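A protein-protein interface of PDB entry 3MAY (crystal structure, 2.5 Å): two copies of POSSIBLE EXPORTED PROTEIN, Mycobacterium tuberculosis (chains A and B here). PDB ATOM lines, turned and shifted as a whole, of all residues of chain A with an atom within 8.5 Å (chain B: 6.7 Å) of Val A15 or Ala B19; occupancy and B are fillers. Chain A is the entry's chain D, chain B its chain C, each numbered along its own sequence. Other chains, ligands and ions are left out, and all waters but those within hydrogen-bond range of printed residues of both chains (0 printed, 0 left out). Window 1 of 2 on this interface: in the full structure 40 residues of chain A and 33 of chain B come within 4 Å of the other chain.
OD1 of Asp B24 is in salt-bridge range of NH2 of Arg A13. O of Ala A12 sits close to O of Ala B19.
Of the printed residues of chain B, Val A15 touches Ala B19. Printed residues of chain A within 4 Å of Ala B19: Ala A12 (3.4 Å), Val A15 (3.8 Å) and Gly A16 (3.6 Å). Of the printed residues of chain A, Gly B16 touches Gly A16. Of the printed residues of chain B, Ala A12 touches Ala B19 (3.4 Å) and Gly B23 (3.8 Å). Of the printed residues of chain B, Ala A19 touches Ala B12. Of the printed residues of chain A, Ile B90 touches Leu A87. The nearest residue of chain A that does not touch Ala B19 is Arg A13 (4.5 Å).
Of the 14 printed residues of chain B, 6 touch a printed residue of chain A. Of the 22 printed residues of chain A, 7 touch a printed residue of chain B. Printed residues of chain A that touch a printed residue of chain B: Ser A9, Ala A12, Arg A13, Val A15, Gly A16, Ala A19 and Leu A87. Among the printed residues, Asp or Glu carboxylates within 4 Å of a Lys or Arg side-chain nitrogen of the other chain: Arg A13 with Asp B24 (3.3 Å).
Ala A12 touches Ala B19, and with the chains exchanged Ala A19 touches Ala B12. Val A15 touches Ala B19, but with the chains exchanged Ala A19 does not touch Val B15 (4.04 Å). Gly A16 touches its own counterpart, Gly B16. Gly A16 touches Ala B19, but with the chains exchanged Ala A19 does not touch Gly B16 (4.002 Å). Positions printed for both chains: 12, 14, 15, 16, 17, 18, 19, 20, 21, 22 and 69. Of the 10 pairs that touch across the chains among the printed residues, 3 have their exchanged pair printed and touching as well.
OD2 of Asp B24 is in salt-bridge range of NZ of Lys B20 (3.0 Å). NH1 of Arg A13 is in salt-bridge range of OE1 of Glu A10 (2.8 Å). The side-chain hydroxyl (OG) of Ser A17 sits at hydrogen-bond distance from the backbone carbonyl oxygen (O) of Arg A13 (3.4 Å).
Gly B23 touches Ser A9 (O to CB, 3.6 Å). Ala A12 touches Gly B23. Arg A13 touches Gly B23. CB of Ala B19 touches CG1 of Val A15, 3.8 Å away. Gly A16 touches Gly B16 (O to CA, 3.6 Å). Gly A16 touches Ala B19 (CA to CB, 3.6 Å). Ala B12 touches Ala A19. Leu A87 touches Ile B90.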
ATOM      1  N   ALA A   8     -16.174   4.454  -0.452  1.00  0.00           N
ATOM      2  CA  ALA A   8     -16.827   5.130   0.666  1.00  0.00           C
ATOM      3  C   ALA A   8     -18.176   5.745   0.285  1.00  0.00           C
ATOM      4  O   ALA A   8     -19.134   5.616   1.008  1.00  0.00           O
ATOM      5  CB  ALA A   8     -15.878   6.184   1.255  1.00  0.00           C
ATOM      6  N   SER A   9     -18.270   6.410  -0.862  1.00  0.00           N
ATOM      7  CA  SER A   9     -19.560   7.029  -1.239  1.00  0.00           C
ATOM      8  C   SER A   9     -20.668   5.993  -1.428  1.00  0.00           C
ATOM      9  O   SER A   9     -21.777   6.208  -0.955  1.00  0.00           O
ATOM     10  CB  SER A   9     -19.411   7.911  -2.463  1.00  0.00           C
ATOM     11  OG  SER A   9     -18.766   7.201  -3.490  1.00  0.00           O
ATOM     12  N   GLU A  10     -20.358   4.860  -2.081  1.00  0.00           N
ATOM     13  CA  GLU A  10     -21.289   3.743  -2.205  1.00  0.00           C
ATOM     14  C   GLU A  10     -21.546   2.980  -0.886  1.00  0.00           C
ATOM     15  O   GLU A  10     -22.689   2.583  -0.602  1.00  0.00           O
ATOM     16  CB  GLU A  10     -20.891   2.786  -3.324  1.00  0.00           C
ATOM     17  CG  GLU A  10     -20.835   3.373  -4.762  1.00  0.00           C
ATOM     18  CD  GLU A  10     -21.882   4.496  -5.068  1.00  0.00           C
ATOM     19  OE1 GLU A  10     -21.450   5.650  -5.405  1.00  0.00           O
ATOM     20  OE2 GLU A  10     -23.121   4.245  -4.969  1.00  0.00           O
ATOM     21  N   VAL A  11     -20.559   2.783  -0.031  1.00  0.00           N
ATOM     22  CA  VAL A  11     -20.968   2.217   1.237  1.00  0.00           C
ATOM     23  C   VAL A  11     -21.885   3.156   1.983  1.00  0.00           C
ATOM     24  O   VAL A  11     -22.930   2.746   2.511  1.00  0.00           O
ATOM     25  CB  VAL A  11     -19.796   1.809   2.167  1.00  0.00           C
ATOM     26  CG1 VAL A  11     -18.634   1.171   1.382  1.00  0.00           C
ATOM     27  CG2 VAL A  11     -19.390   2.966   2.933  1.00  0.00           C
ATOM     28  N   ALA A  12     -21.557   4.442   1.972  1.00  0.00           N
ATOM     29  CA  ALA A  12     -22.432   5.407   2.600  1.00  0.00           C
ATOM     30  C   ALA A  12     -23.834   5.399   2.027  1.00  0.00           C
ATOM     31  O   ALA A  12     -24.812   5.530   2.778  1.00  0.00           O
ATOM     32  CB  ALA A  12     -21.825   6.785   2.566  1.00  0.00           C
ATOM     33  N   ARG A  13     -23.972   5.261   0.716  1.00  0.00           N
ATOM     34  CA  ARG A  13     -25.323   5.202   0.127  1.00  0.00           C
ATOM     35  C   ARG A  13     -26.060   3.936   0.496  1.00  0.00           C
ATOM     36  O   ARG A  13     -27.240   3.990   0.824  1.00  0.00           O
ATOM     37  CB  ARG A  13     -25.325   5.382  -1.396  1.00  0.00           C
ATOM     38  CG  ARG A  13     -25.310   6.872  -1.864  1.00  0.00           C
ATOM     39  CD  ARG A  13     -24.431   7.092  -3.171  1.00  0.00           C
ATOM     40  NE  ARG A  13     -24.485   8.453  -3.708  1.00  0.00           N
ATOM     41  CZ  ARG A  13     -23.743   8.898  -4.741  1.00  0.00           C
ATOM     42  NH1 ARG A  13     -22.856   8.081  -5.348  1.00  0.00           N
ATOM     43  NH2 ARG A  13     -23.869  10.172  -5.178  1.00  0.00           N
ATOM     44  N   THR A  14     -25.381   2.799   0.438  1.00  0.00           N
ATOM     45  CA  THR A  14     -25.960   1.536   0.896  1.00  0.00           C
ATOM     46  C   THR A  14     -26.380   1.676   2.374  1.00  0.00           C
ATOM     47  O   THR A  14     -27.532   1.356   2.737  1.00  0.00           O
ATOM     48  CB  THR A  14     -24.944   0.416   0.799  1.00  0.00           C
ATOM     49  OG1 THR A  14     -24.555   0.251  -0.570  1.00  0.00           O
ATOM     50  CG2 THR A  14     -25.537  -0.886   1.297  1.00  0.00           C
ATOM     51  N   VAL A  15     -25.467   2.181   3.212  1.00  0.00           N
ATOM     52  CA  VAL A  15     -25.796   2.290   4.619  1.00  0.00           C
ATOM     53  C   VAL A  15     -27.015   3.205   4.665  1.00  0.00           C
ATOM     54  O   VAL A  15     -27.969   2.992   5.450  1.00  0.00           O
ATOM     55  CB  VAL A  15     -24.640   2.882   5.431  1.00  0.00           C
ATOM     56  CG1 VAL A  15     -25.180   3.548   6.717  1.00  0.00           C
ATOM     57  CG2 VAL A  15     -23.509   1.829   5.664  1.00  0.00           C
ATOM     58  N   GLY A  16     -27.029   4.185   3.768  1.00  0.00           N
ATOM     59  CA  GLY A  16     -28.122   5.150   3.735  1.00  0.00           C
ATOM     60  C   GLY A  16     -29.428   4.459   3.464  1.00  0.00           C
ATOM     61  O   GLY A  16     -30.418   4.743   4.108  1.00  0.00           O
ATOM     62  N   SER A  17     -29.479   3.542   2.511  1.00  0.00           N
ATOM     63  CA  SER A  17     -30.797   3.127   2.131  1.00  0.00           C
ATOM     64  C   SER A  17     -31.337   1.986   2.996  1.00  0.00           C
ATOM     65  O   SER A  17     -32.572   1.838   3.175  1.00  0.00           O
ATOM     66  CB  SER A  17     -30.886   2.803   0.644  1.00  0.00           C
ATOM     67  OG  SER A  17     -29.898   1.897   0.288  1.00  0.00           O
ATOM     68  N   VAL A  18     -30.407   1.192   3.511  1.00  0.00           N
ATOM     69  CA  VAL A  18     -30.694   0.138   4.469  1.00  0.00           C
ATOM     70  C   VAL A  18     -31.261   0.763   5.715  1.00  0.00           C
ATOM     71  O   VAL A  18     -32.390   0.493   6.052  1.00  0.00           O
ATOM     72  CB  VAL A  18     -29.425  -0.656   4.756  1.00  0.00           C
ATOM     73  CG1 VAL A  18     -29.463  -1.354   6.147  1.00  0.00           C
ATOM     74  CG2 VAL A  18     -29.272  -1.654   3.668  1.00  0.00           C
ATOM     75  N   ALA A  19     -30.525   1.667   6.345  1.00  0.00           N
ATOM     76  CA  ALA A  19     -31.007   2.405   7.516  1.00  0.00           C
ATOM     77  C   ALA A  19     -32.402   3.043   7.344  1.00  0.00           C
ATOM     78  O   ALA A  19     -33.225   3.009   8.259  1.00  0.00           O
ATOM     79  CB  ALA A  19     -29.952   3.429   7.967  1.00  0.00           C
ATOM     80  N   LYS A  20     -32.685   3.620   6.185  1.00  0.00           N
ATOM     81  CA  LYS A  20     -34.005   4.183   5.951  1.00  0.00           C
ATOM     82  C   LYS A  20     -35.082   3.072   5.862  1.00  0.00           C
ATOM     83  O   LYS A  20     -36.267   3.269   6.311  1.00  0.00           O
ATOM     84  CB  LYS A  20     -33.954   5.017   4.682  1.00  0.00           C
ATOM     85  CG  LYS A  20     -35.303   5.340   4.136  1.00  0.00           C
ATOM     86  CD  LYS A  20     -35.215   6.240   2.930  1.00  0.00           C
ATOM     87  CE  LYS A  20     -36.635   6.678   2.585  1.00  0.00           C
ATOM     88  NZ  LYS A  20     -37.499   5.441   2.488  1.00  0.00           N
ATOM     89  N   SER A  21     -34.711   1.908   5.320  1.00  0.00           N
ATOM     90  CA  SER A  21     -35.731   0.847   5.175  1.00  0.00           C
ATOM     91  C   SER A  21     -36.043   0.204   6.545  1.00  0.00           C
ATOM     92  O   SER A  21     -37.164  -0.175   6.850  1.00  0.00           O
ATOM     93  CB  SER A  21     -35.305  -0.187   4.140  1.00  0.00           C
ATOM     94  OG  SER A  21     -34.106  -0.810   4.571  1.00  0.00           O
ATOM     95  N   MET A  22     -35.031   0.102   7.372  1.00  0.00           N
ATOM     96  CA  MET A  22     -35.207  -0.251   8.751  1.00  0.00           C
ATOM     97  C   MET A  22     -36.137   0.712   9.459  1.00  0.00           C
ATOM     98  O   MET A  22     -37.005   0.297  10.224  1.00  0.00           O
ATOM     99  CB  MET A  22     -33.884  -0.111   9.427  1.00  0.00           C
ATOM    100  CG  MET A  22     -33.572  -1.248  10.258  1.00  0.00           C
ATOM    101  SD  MET A  22     -33.139  -2.480   9.028  1.00  0.00           S
ATOM    102  CE  MET A  22     -31.514  -2.968   9.649  1.00  0.00           C
ATOM    103  N   LEU A  69     -33.758  -6.993   5.208  1.00  0.00           N
ATOM    104  CA  LEU A  69     -33.493  -5.574   4.971  1.00  0.00           C
ATOM    105  C   LEU A  69     -32.024  -5.200   5.139  1.00  0.00           C
ATOM    106  O   LEU A  69     -31.550  -4.273   4.498  1.00  0.00           O
ATOM    107  CB  LEU A  69     -34.357  -4.705   5.853  1.00  0.00           C
ATOM    108  CG  LEU A  69     -35.841  -4.665   5.509  1.00  0.00           C
ATOM    109  CD1 LEU A  69     -36.600  -3.861   6.552  1.00  0.00           C
ATOM    110  CD2 LEU A  69     -36.112  -4.150   4.079  1.00  0.00           C
ATOM    111  N   PRO A  72     -28.300  -5.974   1.839  1.00  0.00           N
ATOM    112  CA  PRO A  72     -27.397  -5.164   1.005  1.00  0.00           C
ATOM    113  C   PRO A  72     -26.118  -4.832   1.756  1.00  0.00           C
ATOM    114  O   PRO A  72     -25.019  -4.927   1.215  1.00  0.00           O
ATOM    115  CB  PRO A  72     -28.196  -3.874   0.791  1.00  0.00           C
ATOM    116  CG  PRO A  72     -29.660  -4.336   0.866  1.00  0.00           C
ATOM    117  CD  PRO A  72     -29.617  -5.324   2.002  1.00  0.00           C
ATOM    118  N   LEU A  73     -26.270  -4.484   3.027  1.00  0.00           N
ATOM    119  CA  LEU A  73     -25.132  -4.145   3.834  1.00  0.00           C
ATOM    120  C   LEU A  73     -24.155  -5.279   4.101  1.00  0.00           C
ATOM    121  O   LEU A  73     -22.964  -5.080   3.928  1.00  0.00           O
ATOM    122  CB  LEU A  73     -25.564  -3.448   5.114  1.00  0.00           C
ATOM    123  CG  LEU A  73     -24.498  -2.597   5.820  1.00  0.00           C
ATOM    124  CD1 LEU A  73     -23.787  -1.643   4.868  1.00  0.00           C
ATOM    125  CD2 LEU A  73     -25.182  -1.852   6.922  1.00  0.00           C
ATOM    126  N   THR A  74     -24.632  -6.447   4.511  1.00  0.00           N
ATOM    127  CA  THR A  74     -23.754  -7.598   4.699  1.00  0.00           C
ATOM    128  C   THR A  74     -23.212  -8.119   3.357  1.00  0.00           C
ATOM    129  O   THR A  74     -22.084  -8.609   3.279  1.00  0.00           O
ATOM    130  CB  THR A  74     -24.452  -8.730   5.512  1.00  0.00           C
ATOM    131  OG1 THR A  74     -25.793  -8.329   5.825  1.00  0.00           O
ATOM    132  CG2 THR A  74     -23.706  -8.999   6.840  1.00  0.00           C
ATOM    133  N   LEU A  76     -22.521  -6.067   0.678  1.00  0.00           N
ATOM    134  CA  LEU A  76     -21.396  -5.166   0.412  1.00  0.00           C
ATOM    135  C   LEU A  76     -20.239  -5.517   1.332  1.00  0.00           C
ATOM    136  O   LEU A  76     -19.096  -5.587   0.886  1.00  0.00           O
ATOM    137  CB  LEU A  76     -21.795  -3.699   0.595  1.00  0.00           C
ATOM    138  CG  LEU A  76     -20.975  -2.602  -0.105  1.00  0.00           C
ATOM    139  CD1 LEU A  76     -20.911  -2.734  -1.636  1.00  0.00           C
ATOM    140  CD2 LEU A  76     -21.612  -1.306   0.259  1.00  0.00           C
ATOM    141  N   ILE A  84     -17.304  -5.176   9.358  1.00  0.00           N
ATOM    142  CA  ILE A  84     -18.119  -4.166  10.048  1.00  0.00           C
ATOM    143  C   ILE A  84     -17.433  -3.523  11.268  1.00  0.00           C
ATOM    144  O   ILE A  84     -17.933  -2.539  11.798  1.00  0.00           O
ATOM    145  CB  ILE A  84     -19.567  -4.698  10.404  1.00  0.00           C
ATOM    146  CG1 ILE A  84     -20.017  -5.818   9.426  1.00  0.00           C
ATOM    147  CG2 ILE A  84     -20.587  -3.547  10.369  1.00  0.00           C
ATOM    148  CD1 ILE A  84     -20.684  -7.055  10.096  1.00  0.00           C
ATOM    149  N   LEU A  87     -15.973   0.074   9.866  1.00  0.00           N
ATOM    150  CA  LEU A  87     -16.893   1.164  10.076  1.00  0.00           C
ATOM    151  C   LEU A  87     -16.898   1.568  11.560  1.00  0.00           C
ATOM    152  O   LEU A  87     -16.950   2.760  11.873  1.00  0.00           O
ATOM    153  CB  LEU A  87     -18.299   0.765   9.637  1.00  0.00           C
ATOM    154  CG  LEU A  87     -18.701   0.926   8.174  1.00  0.00           C
ATOM    155  CD1 LEU A  87     -20.207   0.664   8.040  1.00  0.00           C
ATOM    156  CD2 LEU A  87     -18.346   2.321   7.662  1.00  0.00           C
ATOM    157  N   ALA B  12     -33.086   5.749  13.046  1.00  0.00           N
ATOM    158  CA  ALA B  12     -32.759   5.046  11.807  1.00  0.00           C
ATOM    159  C   ALA B  12     -32.975   5.944  10.593  1.00  0.00           C
ATOM    160  O   ALA B  12     -32.106   6.002   9.718  1.00  0.00           O
ATOM    161  CB  ALA B  12     -33.590   3.789  11.663  1.00  0.00           C
ATOM    162  N   THR B  14     -33.159   9.251  10.412  1.00  0.00           N
ATOM    163  CA  THR B  14     -32.173  10.305  10.454  1.00  0.00           C
ATOM    164  C   THR B  14     -30.807   9.793  10.012  1.00  0.00           C
ATOM    165  O   THR B  14     -30.114  10.422   9.159  1.00  0.00           O
ATOM    166  CB  THR B  14     -32.077  10.878  11.851  1.00  0.00           C
ATOM    167  OG1 THR B  14     -33.379  11.393  12.242  1.00  0.00           O
ATOM    168  CG2 THR B  14     -30.991  11.984  11.908  1.00  0.00           C
ATOM    169  N   VAL B  15     -30.407   8.645  10.563  1.00  0.00           N
ATOM    170  CA  VAL B  15     -29.103   8.076  10.218  1.00  0.00           C
ATOM    171  C   VAL B  15     -29.085   7.898   8.696  1.00  0.00           C
ATOM    172  O   VAL B  15     -28.048   8.024   8.028  1.00  0.00           O
ATOM    173  CB  VAL B  15     -28.889   6.686  10.909  1.00  0.00           C
ATOM    174  CG1 VAL B  15     -27.749   5.885  10.293  1.00  0.00           C
ATOM    175  CG2 VAL B  15     -28.678   6.856  12.316  1.00  0.00           C
ATOM    176  N   GLY B  16     -30.240   7.568   8.161  1.00  0.00           N
ATOM    177  CA  GLY B  16     -30.309   7.222   6.743  1.00  0.00           C
ATOM    178  C   GLY B  16     -30.221   8.448   5.861  1.00  0.00           C
ATOM    179  O   GLY B  16     -29.781   8.371   4.750  1.00  0.00           O
ATOM    180  N   SER B  17     -30.633   9.594   6.342  1.00  0.00           N
ATOM    181  CA  SER B  17     -30.456  10.687   5.470  1.00  0.00           C
ATOM    182  C   SER B  17     -29.064  11.314   5.620  1.00  0.00           C
ATOM    183  O   SER B  17     -28.454  11.795   4.644  1.00  0.00           O
ATOM    184  CB  SER B  17     -31.601  11.651   5.596  1.00  0.00           C
ATOM    185  OG  SER B  17     -31.521  12.274   6.810  1.00  0.00           O
ATOM    186  N   VAL B  18     -28.499  11.208   6.800  1.00  0.00           N
ATOM    187  CA  VAL B  18     -27.140  11.572   6.981  1.00  0.00           C
ATOM    188  C   VAL B  18     -26.243  10.762   6.078  1.00  0.00           C
ATOM    189  O   VAL B  18     -25.486  11.333   5.252  1.00  0.00           O
ATOM    190  CB  VAL B  18     -26.696  11.494   8.446  1.00  0.00           C
ATOM    191  CG1 VAL B  18     -25.103  11.585   8.509  1.00  0.00           C
ATOM    192  CG2 VAL B  18     -27.398  12.682   9.153  1.00  0.00           C
ATOM    193  N   ALA B  19     -26.310   9.452   6.183  1.00  0.00           N
ATOM    194  CA  ALA B  19     -25.469   8.590   5.327  1.00  0.00           C
ATOM    195  C   ALA B  19     -25.666   8.863   3.836  1.00  0.00           C
ATOM    196  O   ALA B  19     -24.723   8.994   3.081  1.00  0.00           O
ATOM    197  CB  ALA B  19     -25.738   7.112   5.650  1.00  0.00           C
ATOM    198  N   LYS B  20     -26.905   8.969   3.391  1.00  0.00           N
ATOM    199  CA  LYS B  20     -27.116   9.253   1.985  1.00  0.00           C
ATOM    200  C   LYS B  20     -26.483  10.570   1.617  1.00  0.00           C
ATOM    201  O   LYS B  20     -25.788  10.681   0.647  1.00  0.00           O
ATOM    202  CB  LYS B  20     -28.592   9.285   1.708  1.00  0.00           C
ATOM    203  CG  LYS B  20     -28.895   9.301   0.287  1.00  0.00           C
ATOM    204  CD  LYS B  20     -30.281   9.854   0.067  1.00  0.00           C
ATOM    205  CE  LYS B  20     -30.488  10.018  -1.424  1.00  0.00           C
ATOM    206  NZ  LYS B  20     -29.345  10.858  -1.930  1.00  0.00           N
ATOM    207  N   SER B  21     -26.649  11.582   2.438  1.00  0.00           N
ATOM    208  CA  SER B  21     -26.113  12.839   2.020  1.00  0.00           C
ATOM    209  C   SER B  21     -24.611  12.843   2.194  1.00  0.00           C
ATOM    210  O   SER B  21     -23.914  13.439   1.366  1.00  0.00           O
ATOM    211  CB  SER B  21     -26.836  13.970   2.697  1.00  0.00           C
ATOM    212  OG  SER B  21     -26.543  13.919   4.062  1.00  0.00           O
ATOM    213  N   MET B  22     -24.063  12.100   3.158  1.00  0.00           N
ATOM    214  CA  MET B  22     -22.597  11.870   3.111  1.00  0.00           C
ATOM    215  C   MET B  22     -22.100  11.154   1.844  1.00  0.00           C
ATOM    216  O   MET B  22     -20.974  11.477   1.328  1.00  0.00           O
ATOM    217  CB  MET B  22     -22.037  11.192   4.355  1.00  0.00           C
ATOM    218  CG  MET B  22     -20.521  10.843   4.291  1.00  0.00           C
ATOM    219  SD  MET B  22     -19.947  10.176   5.898  1.00  0.00           S
ATOM    220  CE  MET B  22     -18.256   9.529   5.583  1.00  0.00           C
ATOM    221  N   GLY B  23     -22.896  10.220   1.313  1.00  0.00           N
ATOM    222  CA  GLY B  23     -22.531   9.595   0.050  1.00  0.00           C
ATOM    223  C   GLY B  23     -22.543  10.633  -1.080  1.00  0.00           C
ATOM    224  O   GLY B  23     -21.609  10.691  -1.890  1.00  0.00           O
ATOM    225  N   ASP B  24     -23.591  11.460  -1.152  1.00  0.00           N
ATOM    226  CA  ASP B  24     -23.608  12.558  -2.111  1.00  0.00           C
ATOM    227  C   ASP B  24     -22.395  13.505  -1.974  1.00  0.00           C
ATOM    228  O   ASP B  24     -21.797  13.892  -2.976  1.00  0.00           O
ATOM    229  CB  ASP B  24     -24.902  13.364  -1.946  1.00  0.00           C
ATOM    230  CG  ASP B  24     -26.127  12.597  -2.347  1.00  0.00           C
ATOM    231  OD1 ASP B  24     -26.027  11.590  -3.065  1.00  0.00           O
ATOM    232  OD2 ASP B  24     -27.215  13.008  -1.951  1.00  0.00           O
ATOM    233  N   LEU B  69     -23.047  17.830   7.790  1.00  0.00           N
ATOM    234  CA  LEU B  69     -23.850  16.684   7.297  1.00  0.00           C
ATOM    235  C   LEU B  69     -24.416  15.859   8.461  1.00  0.00           C
ATOM    236  O   LEU B  69     -25.534  15.373   8.349  1.00  0.00           O
ATOM    237  CB  LEU B  69     -23.023  15.762   6.409  1.00  0.00           C
ATOM    238  CG  LEU B  69     -22.994  16.393   5.050  1.00  0.00           C
ATOM    239  CD1 LEU B  69     -22.042  15.686   4.171  1.00  0.00           C
ATOM    240  CD2 LEU B  69     -24.445  16.415   4.466  1.00  0.00           C
ATOM    241  N   ILE B  90     -24.293   1.635  14.712  1.00  0.00           N
ATOM    242  CA  ILE B  90     -23.541   0.449  14.315  1.00  0.00           C
ATOM    243  C   ILE B  90     -23.497  -0.567  15.457  1.00  0.00           C
ATOM    244  O   ILE B  90     -23.636  -1.785  15.245  1.00  0.00           O
ATOM    245  CB  ILE B  90     -22.148   0.795  13.764  1.00  0.00           C
ATOM    246  CG1 ILE B  90     -22.271   1.274  12.315  1.00  0.00           C
ATOM    247  CG2 ILE B  90     -21.231  -0.428  13.843  1.00  0.00           C
ATOM    248  CD1 ILE B  90     -20.971   1.519  11.641  1.00  0.00           C
